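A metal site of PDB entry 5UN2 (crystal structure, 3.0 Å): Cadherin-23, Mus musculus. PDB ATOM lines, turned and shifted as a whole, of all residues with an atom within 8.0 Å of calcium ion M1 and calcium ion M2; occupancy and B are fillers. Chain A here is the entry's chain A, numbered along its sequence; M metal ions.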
ATOM      1  N   GLU A 232       6.607  -1.264 -21.594  1.00  0.00           N
ATOM      2  CA  GLU A 232       7.071  -1.312 -22.980  1.00  0.00           C
ATOM      3  C   GLU A 232       7.891  -0.039 -23.348  1.00  0.00           C
ATOM      4  O   GLU A 232       8.792  -0.090 -24.202  1.00  0.00           O
ATOM      5  CB  GLU A 232       5.927  -1.620 -23.975  1.00  0.00           C
ATOM      6  CG  GLU A 232       4.765  -0.638 -23.981  1.00  0.00           C
ATOM      7  CD  GLU A 232       3.816  -0.831 -25.169  1.00  0.00           C
ATOM      8  OE1 GLU A 232       2.579  -0.599 -25.015  1.00  0.00           O
ATOM      9  OE2 GLU A 232       4.315  -1.192 -26.263  1.00  0.00           O
ATOM     10  N   SER A 233       7.642   1.061 -22.644  1.00  0.00           N
ATOM     11  CA  SER A 233       8.414   2.304 -22.801  1.00  0.00           C
ATOM     12  C   SER A 233       9.832   2.302 -22.212  1.00  0.00           C
ATOM     13  O   SER A 233      10.537   3.300 -22.350  1.00  0.00           O
ATOM     14  CB  SER A 233       7.632   3.485 -22.213  1.00  0.00           C
ATOM     15  OG  SER A 233       7.730   3.500 -20.791  1.00  0.00           O
ATOM     16  N   LEU A 293      11.533  -2.373 -26.596  1.00  0.00           N
ATOM     17  CA  LEU A 293      10.405  -3.271 -26.275  1.00  0.00           C
ATOM     18  C   LEU A 293       9.077  -2.742 -26.834  1.00  0.00           C
ATOM     19  O   LEU A 293       8.821  -1.549 -26.784  1.00  0.00           O
ATOM     20  CB  LEU A 293      10.264  -3.400 -24.759  1.00  0.00           C
ATOM     21  CG  LEU A 293      11.489  -3.864 -23.993  1.00  0.00           C
ATOM     22  CD1 LEU A 293      11.291  -3.693 -22.500  1.00  0.00           C
ATOM     23  CD2 LEU A 293      11.788  -5.321 -24.312  1.00  0.00           C
ATOM     24  N   ASN A 294       8.262  -3.649 -27.362  1.00  0.00           N
ATOM     25  CA  ASN A 294       6.907  -3.352 -27.852  1.00  0.00           C
ATOM     26  C   ASN A 294       5.978  -4.451 -27.362  1.00  0.00           C
ATOM     27  O   ASN A 294       6.145  -5.619 -27.753  1.00  0.00           O
ATOM     28  CB  ASN A 294       6.871  -3.277 -29.377  1.00  0.00           C
ATOM     29  CG  ASN A 294       5.510  -2.871 -29.921  1.00  0.00           C
ATOM     30  OD1 ASN A 294       4.631  -2.420 -29.193  1.00  0.00           O
ATOM     31  ND2 ASN A 294       5.334  -3.006 -31.217  1.00  0.00           N
ATOM     32  N   ARG A 295       5.006  -4.096 -26.521  1.00  0.00           N
ATOM     33  CA  ARG A 295       4.033  -5.058 -25.996  1.00  0.00           C
ATOM     34  C   ARG A 295       3.199  -5.689 -27.106  1.00  0.00           C
ATOM     35  O   ARG A 295       2.823  -6.860 -27.040  1.00  0.00           O
ATOM     36  CB  ARG A 295       3.092  -4.388 -24.988  1.00  0.00           C
ATOM     37  CG  ARG A 295       2.030  -5.358 -24.523  1.00  0.00           C
ATOM     38  CD  ARG A 295       1.307  -5.001 -23.251  1.00  0.00           C
ATOM     39  NE  ARG A 295       0.898  -6.258 -22.611  1.00  0.00           N
ATOM     40  CZ  ARG A 295      -0.081  -7.058 -23.044  1.00  0.00           C
ATOM     41  NH1 ARG A 295      -0.327  -8.197 -22.378  1.00  0.00           N
ATOM     42  NH2 ARG A 295      -0.816  -6.754 -24.121  1.00  0.00           N
ATOM     43  N   GLU A 296       2.919  -4.890 -28.121  1.00  0.00           N
ATOM     44  CA  GLU A 296       2.081  -5.293 -29.230  1.00  0.00           C
ATOM     45  C   GLU A 296       2.779  -6.317 -30.135  1.00  0.00           C
ATOM     46  O   GLU A 296       2.125  -6.993 -30.942  1.00  0.00           O
ATOM     47  CB  GLU A 296       1.645  -4.055 -30.013  1.00  0.00           C
ATOM     48  CG  GLU A 296       0.588  -3.233 -29.292  1.00  0.00           C
ATOM     49  CD  GLU A 296       1.092  -2.543 -28.036  1.00  0.00           C
ATOM     50  OE1 GLU A 296       0.531  -2.817 -26.947  1.00  0.00           O
ATOM     51  OE2 GLU A 296       2.016  -1.705 -28.116  1.00  0.00           O
ATOM     52  N   LEU A 297       4.105  -6.415 -29.994  1.00  0.00           N
ATOM     53  CA  LEU A 297       4.898  -7.474 -30.577  1.00  0.00           C
ATOM     54  C   LEU A 297       5.104  -8.629 -29.618  1.00  0.00           C
ATOM     55  O   LEU A 297       4.763  -9.773 -29.923  1.00  0.00           O
ATOM     56  CB  LEU A 297       6.247  -6.927 -31.032  1.00  0.00           C
ATOM     57  CG  LEU A 297       7.167  -7.854 -31.830  1.00  0.00           C
ATOM     58  CD1 LEU A 297       6.485  -8.312 -33.096  1.00  0.00           C
ATOM     59  CD2 LEU A 297       8.460  -7.102 -32.124  1.00  0.00           C
ATOM     60  N   ILE A 330       5.418  -7.967 -19.975  1.00  0.00           N
ATOM     61  CA  ILE A 330       5.513  -6.621 -20.510  1.00  0.00           C
ATOM     62  C   ILE A 330       4.192  -5.860 -20.338  1.00  0.00           C
ATOM     63  O   ILE A 330       3.144  -6.300 -20.856  1.00  0.00           O
ATOM     64  CB  ILE A 330       5.924  -6.601 -22.000  1.00  0.00           C
ATOM     65  CG1 ILE A 330       7.280  -7.285 -22.205  1.00  0.00           C
ATOM     66  CG2 ILE A 330       5.974  -5.177 -22.538  1.00  0.00           C
ATOM     67  CD1 ILE A 330       8.473  -6.477 -21.751  1.00  0.00           C
ATOM     68  N   LEU A 331       4.289  -4.701 -19.654  1.00  0.00           N
ATOM     69  CA  LEU A 331       3.158  -3.804 -19.377  1.00  0.00           C
ATOM     70  C   LEU A 331       2.796  -2.827 -20.529  1.00  0.00           C
ATOM     71  O   LEU A 331       3.688  -2.335 -21.235  1.00  0.00           O
ATOM     72  CB  LEU A 331       3.427  -3.027 -18.086  1.00  0.00           C
ATOM     73  CG  LEU A 331       3.664  -3.863 -16.829  1.00  0.00           C
ATOM     74  CD1 LEU A 331       4.143  -2.973 -15.692  1.00  0.00           C
ATOM     75  CD2 LEU A 331       2.402  -4.605 -16.455  1.00  0.00           C
ATOM     76  N   ASP A 332       1.496  -2.554 -20.698  1.00  0.00           N
ATOM     77  CA  ASP A 332       0.991  -1.811 -21.872  1.00  0.00           C
ATOM     78  C   ASP A 332       1.102  -0.329 -21.651  1.00  0.00           C
ATOM     79  O   ASP A 332       0.933   0.141 -20.551  1.00  0.00           O
ATOM     80  CB  ASP A 332      -0.472  -2.144 -22.176  1.00  0.00           C
ATOM     81  CG  ASP A 332      -0.935  -1.581 -23.523  1.00  0.00           C
ATOM     82  OD1 ASP A 332      -0.089  -1.354 -24.418  1.00  0.00           O
ATOM     83  OD2 ASP A 332      -2.161  -1.357 -23.689  1.00  0.00           O
ATOM     84  N   VAL A 333       1.386   0.410 -22.711  1.00  0.00           N
ATOM     85  CA  VAL A 333       1.311   1.869 -22.661  1.00  0.00           C
ATOM     86  C   VAL A 333       0.290   2.310 -23.705  1.00  0.00           C
ATOM     87  O   VAL A 333       0.310   1.799 -24.835  1.00  0.00           O
ATOM     88  CB  VAL A 333       2.704   2.510 -22.850  1.00  0.00           C
ATOM     89  CG1 VAL A 333       2.604   4.031 -22.912  1.00  0.00           C
ATOM     90  CG2 VAL A 333       3.643   2.094 -21.727  1.00  0.00           C
ATOM     91  N   ASN A 334      -0.622   3.211 -23.317  1.00  0.00           N
ATOM     92  CA  ASN A 334      -1.683   3.706 -24.203  1.00  0.00           C
ATOM     93  C   ASN A 334      -2.268   5.066 -23.692  1.00  0.00           C
ATOM     94  O   ASN A 334      -1.774   5.623 -22.711  1.00  0.00           O
ATOM     95  CB  ASN A 334      -2.735   2.618 -24.455  1.00  0.00           C
ATOM     96  CG  ASN A 334      -3.416   2.156 -23.188  1.00  0.00           C
ATOM     97  OD1 ASN A 334      -4.337   2.814 -22.690  1.00  0.00           O
ATOM     98  ND2 ASN A 334      -2.994   1.013 -22.669  1.00  0.00           N
ATOM     99  N   ASP A 335      -3.302   5.561 -24.368  1.00  0.00           N
ATOM    100  CA  ASP A 335      -3.733   6.979 -24.288  1.00  0.00           C
ATOM    101  C   ASP A 335      -4.320   7.383 -22.927  1.00  0.00           C
ATOM    102  O   ASP A 335      -5.537   7.420 -22.744  1.00  0.00           O
ATOM    103  CB  ASP A 335      -4.733   7.301 -25.428  1.00  0.00           C
ATOM    104  CG  ASP A 335      -4.245   6.828 -26.807  1.00  0.00           C
ATOM    105  OD1 ASP A 335      -3.072   6.366 -26.932  1.00  0.00           O
ATOM    106  OD2 ASP A 335      -5.030   6.901 -27.775  1.00  0.00           O
HETATM  107 CA    CA M   1       0.585  -0.117 -26.327  1.00  0.00          CA
HETATM  108 CA    CA M   2       4.293  -0.381 -28.508  1.00  0.00          CA
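Calcium ion M1 is bound by the side-chain carboxylate (OD1) of Asp 332 (2.4 Å), the side-chain carboxylate (OE1) of Glu 232 (2.4 Å), the backbone carbonyl oxygen (O) of Val 333 (2.4 Å), the side-chain carboxylate (OE1) of Glu 296 (2.8 Å) and the side-chain carboxylate (OE2) of Glu 296 (2.8 Å).
Calcium ion M1 has five donor atoms within binding distance.
The side-chain carboxylate of Asp 332 sits at hydrogen-bond distance from the side-chain amide nitrogen of Asn 334, at 2.7 Å.
The backbone NH (N) of Glu 232 is in hydrogen-bond range of the backbone carbonyl oxygen (O) of Leu 331 (3.1 Å).
The backbone NH of Arg 295 lies close to the side-chain carboxylate of Glu 232 (3.0 Å).
Calcium ion M2 is bound by the side-chain amide oxygen (OD1) of Asn 294, the side-chain carboxylate (OE2) of Glu 232 and the side-chain carboxylate (OE2) of Glu 296.
Calcium ion M2 has three donor atoms within binding distance.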
